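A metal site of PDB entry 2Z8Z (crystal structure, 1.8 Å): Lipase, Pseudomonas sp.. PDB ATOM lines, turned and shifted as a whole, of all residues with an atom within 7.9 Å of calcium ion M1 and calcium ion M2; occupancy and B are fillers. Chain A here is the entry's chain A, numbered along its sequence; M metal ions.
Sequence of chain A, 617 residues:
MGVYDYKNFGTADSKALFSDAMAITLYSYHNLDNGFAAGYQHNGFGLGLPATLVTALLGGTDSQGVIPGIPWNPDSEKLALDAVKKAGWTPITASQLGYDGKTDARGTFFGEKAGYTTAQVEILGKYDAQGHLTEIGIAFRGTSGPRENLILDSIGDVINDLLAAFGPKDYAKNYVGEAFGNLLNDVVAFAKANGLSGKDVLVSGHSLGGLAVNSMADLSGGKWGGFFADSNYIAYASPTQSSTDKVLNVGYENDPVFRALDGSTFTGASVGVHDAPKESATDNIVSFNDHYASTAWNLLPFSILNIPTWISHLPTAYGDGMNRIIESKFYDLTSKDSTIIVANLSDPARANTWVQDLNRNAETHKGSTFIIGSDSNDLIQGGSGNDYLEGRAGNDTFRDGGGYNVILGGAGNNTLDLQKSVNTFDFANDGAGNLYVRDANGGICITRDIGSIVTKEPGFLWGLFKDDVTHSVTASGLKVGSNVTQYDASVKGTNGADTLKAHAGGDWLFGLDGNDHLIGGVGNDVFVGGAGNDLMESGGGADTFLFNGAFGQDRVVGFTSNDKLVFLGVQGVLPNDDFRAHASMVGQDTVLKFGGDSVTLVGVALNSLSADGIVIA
The backbone carbonyl oxygen of Leu 408 is in hydrogen-bond range of the backbone NH of Gly 391, at 3.0 Å. ND2 of Asn 414 is in hydrogen-bond range of O of Asp 449 (2.8 Å). N of Ser 376 sits at hydrogen-bond distance from OG of Ser 374 (3.0 Å). The side-chain amide nitrogen of Asn 414 lies within hydrogen-bond range of the backbone carbonyl oxygen of Gly 410 (3.1 Å). The guanidinium group (NE) of Arg 392 lies within salt-bridge range of the side-chain carboxylate (OD1) of Asp 375, at 2.9 Å. O of Asp 378 sits at hydrogen-bond distance from N of Thr 397, at 2.9 Å. ND2 of Asn 414 sits at hydrogen-bond distance from O of Gly 412 (3.4 Å). N of Thr 415 lies within hydrogen-bond range of O of Asp 396, 2.9 Å away.
Gly 410 touches calcium ion M1. Along chain A the residues within 4 Å of calcium ion M1 span positions 392 to 414. The nearest printed residue that does not touch calcium ion M1 is Gly 391 (4.2 Å).
Within 4 Å of calcium ion M2: Ser 374, Ser 376, Asp 378, Gly 391, Arg 392, Ala 393 and Asp 396. The nearest printed residue that does not touch calcium ion M2 is Asp 375 (4.1 Å).
Calcium ion M1 is bound by the side-chain carboxylate (OD2) of Asp 396, the backbone carbonyl oxygen (O) of Ala 411, the backbone carbonyl oxygen (O) of Gly 394, the backbone carbonyl oxygen (O) of Arg 392, the backbone carbonyl oxygen (O) of Gly 409 and the side-chain amide oxygen (OD1) of Asn 414.
Calcium ion M2 is bound by the side-chain carboxylate (OD2) of Asp 378 (2.2 Å), the backbone carbonyl oxygen (O) of Ala 393 (2.2 Å), the backbone carbonyl oxygen (O) of Ser 376 (2.3 Å), the backbone carbonyl oxygen (O) of Gly 391 (2.3 Å), the backbone carbonyl oxygen (O) of Ser 374 (2.4 Å) and the side-chain carboxylate (OD1) of Asp 396 (2.5 Å). Slightly farther from calcium ion M2 lies the side-chain carboxylate (OD2) of Asp 396 (3.0 Å).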
ATOM      1  N   ALA A 343      19.874  35.086  12.937  1.00  0.00           N
ATOM      2  CA  ALA A 343      19.107  34.513  11.875  1.00  0.00           C
ATOM      3  C   ALA A 343      18.120  35.560  11.340  1.00  0.00           C
ATOM      4  O   ALA A 343      17.103  35.894  12.007  1.00  0.00           O
ATOM      5  CB  ALA A 343      18.356  33.286  12.384  1.00  0.00           C
ATOM      6  N   ARG A 350      14.326  30.524   4.827  1.00  0.00           N
ATOM      7  CA  ARG A 350      14.491  29.880   6.130  1.00  0.00           C
ATOM      8  C   ARG A 350      14.260  28.377   6.017  1.00  0.00           C
ATOM      9  O   ARG A 350      14.859  27.562   6.770  1.00  0.00           O
ATOM     10  CB  ARG A 350      13.507  30.484   7.151  1.00  0.00           C
ATOM     11  CG  ARG A 350      13.819  30.062   8.570  1.00  0.00           C
ATOM     12  CD  ARG A 350      12.917  30.753   9.550  1.00  0.00           C
ATOM     13  NE  ARG A 350      11.523  30.615   9.154  1.00  0.00           N
ATOM     14  CZ  ARG A 350      10.682  31.605   8.892  1.00  0.00           C
ATOM     15  NH1 ARG A 350      11.039  32.876   9.012  1.00  0.00           N
ATOM     16  NH2 ARG A 350       9.442  31.296   8.542  1.00  0.00           N
ATOM     17  N   ILE A 372      21.899  32.942  16.985  1.00  0.00           N
ATOM     18  CA  ILE A 372      20.584  33.220  17.551  1.00  0.00           C
ATOM     19  C   ILE A 372      19.495  33.000  16.498  1.00  0.00           C
ATOM     20  O   ILE A 372      19.438  33.698  15.482  1.00  0.00           O
ATOM     21  CB  ILE A 372      20.469  34.685  18.052  1.00  0.00           C
ATOM     22  CG1 ILE A 372      21.646  35.053  18.966  1.00  0.00           C
ATOM     23  CG2 ILE A 372      19.197  34.903  18.859  1.00  0.00           C
ATOM     24  CD1 ILE A 372      21.862  34.089  20.030  1.00  0.00           C
ATOM     25  N   GLY A 373      18.575  32.115  16.803  1.00  0.00           N
ATOM     26  CA  GLY A 373      17.475  31.813  15.869  1.00  0.00           C
ATOM     27  C   GLY A 373      16.336  32.810  15.836  1.00  0.00           C
ATOM     28  O   GLY A 373      16.383  33.841  16.501  1.00  0.00           O
ATOM     29  N   SER A 374      15.287  32.499  15.042  1.00  0.00           N
ATOM     30  CA  SER A 374      14.053  33.272  14.958  1.00  0.00           C
ATOM     31  C   SER A 374      12.985  32.558  15.724  1.00  0.00           C
ATOM     32  O   SER A 374      13.175  31.424  16.157  1.00  0.00           O
ATOM     33  CB  SER A 374      13.567  33.398  13.520  1.00  0.00           C
ATOM     34  OG  SER A 374      13.076  32.181  13.003  1.00  0.00           O
ATOM     35  N   ASP A 375      11.832  33.182  15.836  1.00  0.00           N
ATOM     36  CA  ASP A 375      10.710  32.519  16.440  1.00  0.00           C
ATOM     37  C   ASP A 375       9.999  31.497  15.562  1.00  0.00           C
ATOM     38  O   ASP A 375       9.010  30.892  16.016  1.00  0.00           O
ATOM     39  CB  ASP A 375       9.783  33.560  17.000  1.00  0.00           C
ATOM     40  CG  ASP A 375      10.316  34.119  18.328  1.00  0.00           C
ATOM     41  OD1 ASP A 375      11.020  33.409  19.108  1.00  0.00           O
ATOM     42  OD2 ASP A 375       9.980  35.218  18.575  1.00  0.00           O
ATOM     43  N   SER A 376      10.525  31.265  14.374  1.00  0.00           N
ATOM     44  CA  SER A 376       9.979  30.222  13.497  1.00  0.00           C
ATOM     45  C   SER A 376      10.930  29.021  13.414  1.00  0.00           C
ATOM     46  O   SER A 376      11.929  28.912  14.171  1.00  0.00           O
ATOM     47  CB  SER A 376       9.731  30.828  12.137  1.00  0.00           C
ATOM     48  OG  SER A 376       8.870  31.950  12.269  1.00  0.00           O
ATOM     49  N   ASN A 377      10.610  28.069  12.536  1.00  0.00           N
ATOM     50  CA  ASN A 377      11.425  26.880  12.376  1.00  0.00           C
ATOM     51  C   ASN A 377      12.732  27.193  11.680  1.00  0.00           C
ATOM     52  O   ASN A 377      12.710  27.589  10.506  1.00  0.00           O
ATOM     53  CB  ASN A 377      10.666  25.871  11.484  1.00  0.00           C
ATOM     54  CG  ASN A 377       9.393  25.418  12.106  1.00  0.00           C
ATOM     55  OD1 ASN A 377       9.072  25.827  13.184  1.00  0.00           O
ATOM     56  ND2 ASN A 377       8.662  24.539  11.407  1.00  0.00           N
ATOM     57  N   ASP A 378      13.847  27.022  12.395  1.00  0.00           N
ATOM     58  CA  ASP A 378      15.189  27.315  11.886  1.00  0.00           C
ATOM     59  C   ASP A 378      15.996  26.048  11.652  1.00  0.00           C
ATOM     60  O   ASP A 378      15.767  25.062  12.347  1.00  0.00           O
ATOM     61  CB  ASP A 378      15.929  28.162  12.963  1.00  0.00           C
ATOM     62  CG  ASP A 378      15.189  29.447  13.297  1.00  0.00           C
ATOM     63  OD1 ASP A 378      14.956  30.230  12.334  1.00  0.00           O
ATOM     64  OD2 ASP A 378      14.832  29.682  14.506  1.00  0.00           O
ATOM     65  N   LEU A 379      16.971  26.129  10.727  1.00  0.00           N
ATOM     66  CA  LEU A 379      18.055  25.180  10.472  1.00  0.00           C
ATOM     67  C   LEU A 379      19.294  25.954  10.898  1.00  0.00           C
ATOM     68  O   LEU A 379      19.615  26.986  10.319  1.00  0.00           O
ATOM     69  CB  LEU A 379      18.187  24.779   8.968  1.00  0.00           C
ATOM     70  CG  LEU A 379      16.871  24.240   8.374  1.00  0.00           C
ATOM     71  CD1 LEU A 379      17.003  24.028   6.885  1.00  0.00           C
ATOM     72  CD2 LEU A 379      16.487  22.964   9.065  1.00  0.00           C
ATOM     73  N   ILE A 380      19.894  25.488  11.992  1.00  0.00           N
ATOM     74  CA  ILE A 380      21.052  26.131  12.596  1.00  0.00           C
ATOM     75  C   ILE A 380      22.291  25.208  12.572  1.00  0.00           C
ATOM     76  O   ILE A 380      22.263  24.071  13.083  1.00  0.00           O
ATOM     77  CB  ILE A 380      20.697  26.600  14.028  1.00  0.00           C
ATOM     78  CG1 ILE A 380      19.617  27.720  13.995  1.00  0.00           C
ATOM     79  CG2 ILE A 380      21.924  27.066  14.736  1.00  0.00           C
ATOM     80  CD1 ILE A 380      19.017  28.051  15.272  1.00  0.00           C
ATOM     81  N   GLU A 390      20.954  28.867  19.731  1.00  0.00           N
ATOM     82  CA  GLU A 390      19.688  29.159  20.407  1.00  0.00           C
ATOM     83  C   GLU A 390      18.566  29.172  19.359  1.00  0.00           C
ATOM     84  O   GLU A 390      18.555  30.004  18.446  1.00  0.00           O
ATOM     85  CB  GLU A 390      19.757  30.513  21.134  1.00  0.00           C
ATOM     86  CG  GLU A 390      18.476  30.802  21.922  1.00  0.00           C
ATOM     87  CD  GLU A 390      18.585  32.057  22.765  1.00  0.00           C
ATOM     88  OE1 GLU A 390      19.143  33.071  22.189  1.00  0.00           O
ATOM     89  OE2 GLU A 390      18.101  32.039  23.936  1.00  0.00           O
ATOM     90  N   GLY A 391      17.642  28.222  19.502  1.00  0.00           N
ATOM     91  CA  GLY A 391      16.526  28.042  18.585  1.00  0.00           C
ATOM     92  C   GLY A 391      15.358  28.996  18.762  1.00  0.00           C
ATOM     93  O   GLY A 391      14.753  29.372  17.754  1.00  0.00           O
ATOM     94  N   ARG A 392      15.101  29.422  19.993  1.00  0.00           N
ATOM     95  CA  ARG A 392      13.892  30.117  20.350  1.00  0.00           C
ATOM     96  C   ARG A 392      12.659  29.292  19.889  1.00  0.00           C
ATOM     97  O   ARG A 392      12.779  28.094  19.773  1.00  0.00           O
ATOM     98  CB  ARG A 392      13.885  31.566  19.782  1.00  0.00           C
ATOM     99  CG  ARG A 392      15.110  32.419  20.144  1.00  0.00           C
ATOM    100  CD  ARG A 392      15.019  33.863  19.494  1.00  0.00           C
ATOM    101  NE  ARG A 392      13.680  34.448  19.700  1.00  0.00           N
ATOM    102  CZ  ARG A 392      13.384  35.327  20.659  1.00  0.00           C
ATOM    103  NH1 ARG A 392      14.318  35.733  21.492  1.00  0.00           N
ATOM    104  NH2 ARG A 392      12.197  35.869  20.754  1.00  0.00           N
ATOM    105  N   ALA A 393      11.500  29.928  19.677  1.00  0.00           N
ATOM    106  CA  ALA A 393      10.313  29.185  19.314  1.00  0.00           C
ATOM    107  C   ALA A 393      10.452  28.601  17.945  1.00  0.00           C
ATOM    108  O   ALA A 393      11.465  28.851  17.169  1.00  0.00           O
ATOM    109  CB  ALA A 393       9.081  30.079  19.413  1.00  0.00           C
ATOM    110  N   GLY A 394       9.464  27.782  17.592  1.00  0.00           N
ATOM    111  CA  GLY A 394       9.535  27.093  16.337  1.00  0.00           C
ATOM    112  C   GLY A 394      10.261  25.765  16.536  1.00  0.00           C
ATOM    113  O   GLY A 394      10.905  25.518  17.574  1.00  0.00           O
ATOM    114  N   ASN A 395      10.074  24.876  15.573  1.00  0.00           N
ATOM    115  CA  ASN A 395      10.643  23.528  15.582  1.00  0.00           C
ATOM    116  C   ASN A 395      11.977  23.713  14.885  1.00  0.00           C
ATOM    117  O   ASN A 395      12.038  23.891  13.677  1.00  0.00           O
ATOM    118  CB  ASN A 395       9.804  22.579  14.769  1.00  0.00           C
ATOM    119  CG  ASN A 395       8.448  22.292  15.419  1.00  0.00           C
ATOM    120  OD1 ASN A 395       8.219  22.633  16.574  1.00  0.00           O
ATOM    121  ND2 ASN A 395       7.536  21.692  14.643  1.00  0.00           N
ATOM    122  N   ASP A 396      13.060  23.654  15.665  1.00  0.00           N
ATOM    123  CA  ASP A 396      14.400  23.980  15.129  1.00  0.00           C
ATOM    124  C   ASP A 396      15.205  22.723  14.977  1.00  0.00           C
ATOM    125  O   ASP A 396      15.107  21.837  15.819  1.00  0.00           O
ATOM    126  CB  ASP A 396      15.118  24.949  16.112  1.00  0.00           C
ATOM    127  CG  ASP A 396      14.315  26.194  16.323  1.00  0.00           C
ATOM    128  OD1 ASP A 396      14.003  26.800  15.277  1.00  0.00           O
ATOM    129  OD2 ASP A 396      13.886  26.494  17.466  1.00  0.00           O
ATOM    130  N   THR A 397      16.058  22.692  13.933  1.00  0.00           N
ATOM    131  CA  THR A 397      16.952  21.598  13.711  1.00  0.00           C
ATOM    132  C   THR A 397      18.402  22.096  13.785  1.00  0.00           C
ATOM    133  O   THR A 397      18.712  23.105  13.155  1.00  0.00           O
ATOM    134  CB  THR A 397      16.711  20.940  12.356  1.00  0.00           C
ATOM    135  OG1 THR A 397      15.329  20.511  12.310  1.00  0.00           O
ATOM    136  CG2 THR A 397      17.584  19.761  12.235  1.00  0.00           C
ATOM    137  N   PHE A 398      19.215  21.421  14.602  1.00  0.00           N
ATOM    138  CA  PHE A 398      20.617  21.812  14.801  1.00  0.00           C
ATOM    139  C   PHE A 398      21.581  20.783  14.270  1.00  0.00           C
ATOM    140  O   PHE A 398      21.383  19.580  14.406  1.00  0.00           O
ATOM    141  CB  PHE A 398      20.926  22.025  16.281  1.00  0.00           C
ATOM    142  CG  PHE A 398      20.028  23.003  16.976  1.00  0.00           C
ATOM    143  CD1 PHE A 398      20.369  24.335  17.104  1.00  0.00           C
ATOM    144  CD2 PHE A 398      18.832  22.578  17.540  1.00  0.00           C
ATOM    145  CE1 PHE A 398      19.482  25.232  17.814  1.00  0.00           C
ATOM    146  CE2 PHE A 398      18.003  23.441  18.210  1.00  0.00           C
ATOM    147  CZ  PHE A 398      18.342  24.801  18.348  1.00  0.00           C
ATOM    148  N   LEU A 408      20.326  25.183  22.901  1.00  0.00           N
ATOM    149  CA  LEU A 408      19.052  25.420  23.577  1.00  0.00           C
ATOM    150  C   LEU A 408      17.937  25.319  22.521  1.00  0.00           C
ATOM    151  O   LEU A 408      17.746  26.193  21.714  1.00  0.00           O
ATOM    152  CB  LEU A 408      19.003  26.768  24.245  1.00  0.00           C
ATOM    153  CG  LEU A 408      20.128  27.033  25.301  1.00  0.00           C
ATOM    154  CD1 LEU A 408      20.081  28.459  25.854  1.00  0.00           C
ATOM    155  CD2 LEU A 408      19.930  26.021  26.413  1.00  0.00           C
ATOM    156  N   GLY A 409      17.197  24.237  22.563  1.00  0.00           N
ATOM    157  CA  GLY A 409      16.097  24.124  21.645  1.00  0.00           C
ATOM    158  C   GLY A 409      15.011  25.168  21.744  1.00  0.00           C
ATOM    159  O   GLY A 409      14.354  25.434  20.734  1.00  0.00           O
ATOM    160  N   GLY A 410      14.762  25.695  22.942  1.00  0.00           N
ATOM    161  CA  GLY A 410      13.606  26.551  23.228  1.00  0.00           C
ATOM    162  C   GLY A 410      12.266  25.848  23.091  1.00  0.00           C
ATOM    163  O   GLY A 410      12.186  24.602  23.141  1.00  0.00           O
ATOM    164  N   ALA A 411      11.206  26.629  22.937  1.00  0.00           N
ATOM    165  CA  ALA A 411       9.891  26.118  22.621  1.00  0.00           C
ATOM    166  C   ALA A 411       9.894  25.305  21.370  1.00  0.00           C
ATOM    167  O   ALA A 411      10.808  25.344  20.563  1.00  0.00           O
ATOM    168  CB  ALA A 411       8.884  27.250  22.515  1.00  0.00           C
ATOM    169  N   GLY A 412       8.863  24.498  21.193  1.00  0.00           N
ATOM    170  CA  GLY A 412       8.755  23.669  19.989  1.00  0.00           C
ATOM    171  C   GLY A 412       9.272  22.230  20.107  1.00  0.00           C
ATOM    172  O   GLY A 412       9.752  21.795  21.157  1.00  0.00           O
ATOM    173  N   ASN A 413       9.169  21.516  18.992  1.00  0.00           N
ATOM    174  CA  ASN A 413       9.729  20.167  18.867  1.00  0.00           C
ATOM    175  C   ASN A 413      11.013  20.293  18.096  1.00  0.00           C
ATOM    176  O   ASN A 413      10.999  20.507  16.864  1.00  0.00           O
ATOM    177  CB  ASN A 413       8.769  19.237  18.122  1.00  0.00           C
ATOM    178  CG  ASN A 413       7.474  19.079  18.839  1.00  0.00           C
ATOM    179  OD1 ASN A 413       7.417  18.936  20.070  1.00  0.00           O
ATOM    180  ND2 ASN A 413       6.382  19.154  18.072  1.00  0.00           N
ATOM    181  N   ASN A 414      12.120  20.161  18.818  1.00  0.00           N
ATOM    182  CA  ASN A 414      13.426  20.424  18.273  1.00  0.00           C
ATOM    183  C   ASN A 414      14.240  19.155  18.071  1.00  0.00           C
ATOM    184  O   ASN A 414      14.067  18.206  18.817  1.00  0.00           O
ATOM    185  CB  ASN A 414      14.210  21.404  19.212  1.00  0.00           C
ATOM    186  CG  ASN A 414      13.374  22.590  19.617  1.00  0.00           C
ATOM    187  OD1 ASN A 414      13.037  23.412  18.781  1.00  0.00           O
ATOM    188  ND2 ASN A 414      13.033  22.681  20.918  1.00  0.00           N
ATOM    189  N   THR A 415      15.187  19.212  17.145  1.00  0.00           N
ATOM    190  CA  THR A 415      16.007  18.110  16.717  1.00  0.00           C
ATOM    191  C   THR A 415      17.502  18.451  16.626  1.00  0.00           C
ATOM    192  O   THR A 415      17.889  19.520  16.154  1.00  0.00           O
ATOM    193  CB  THR A 415      15.525  17.693  15.288  1.00  0.00           C
ATOM    194  OG1 THR A 415      14.129  17.356  15.386  1.00  0.00           O
ATOM    195  CG2 THR A 415      16.287  16.481  14.748  1.00  0.00           C
ATOM    196  N   ASP A 449      15.780  20.945  25.810  1.00  0.00           N
ATOM    197  CA  ASP A 449      14.566  20.999  24.969  1.00  0.00           C
ATOM    198  C   ASP A 449      14.792  20.400  23.597  1.00  0.00           C
ATOM    199  O   ASP A 449      14.218  20.839  22.653  1.00  0.00           O
ATOM    200  CB  ASP A 449      14.075  22.461  24.906  1.00  0.00           C
ATOM    201  CG  ASP A 449      13.725  22.996  26.281  1.00  0.00           C
ATOM    202  OD1 ASP A 449      12.887  22.368  26.952  1.00  0.00           O
ATOM    203  OD2 ASP A 449      14.278  23.997  26.728  1.00  0.00           O
ATOM    204  N   ILE A 450      15.576  19.335  23.527  1.00  0.00           N
ATOM    205  CA  ILE A 450      15.759  18.617  22.283  1.00  0.00           C
ATOM    206  C   ILE A 450      15.113  17.220  22.479  1.00  0.00           C
ATOM    207  O   ILE A 450      15.551  16.426  23.317  1.00  0.00           O
ATOM    208  CB  ILE A 450      17.235  18.658  21.806  1.00  0.00           C
ATOM    209  CG1 ILE A 450      17.426  20.070  21.147  1.00  0.00           C
ATOM    210  CG2 ILE A 450      17.462  17.442  20.840  1.00  0.00           C
ATOM    211  CD1 ILE A 450      18.747  20.563  20.864  1.00  0.00           C
HETATM  212 CA    CA M   1      12.554  25.833  19.182  1.00  0.00          CA
HETATM  213 CA    CA M   2      13.321  29.058  15.966  1.00  0.00          CA
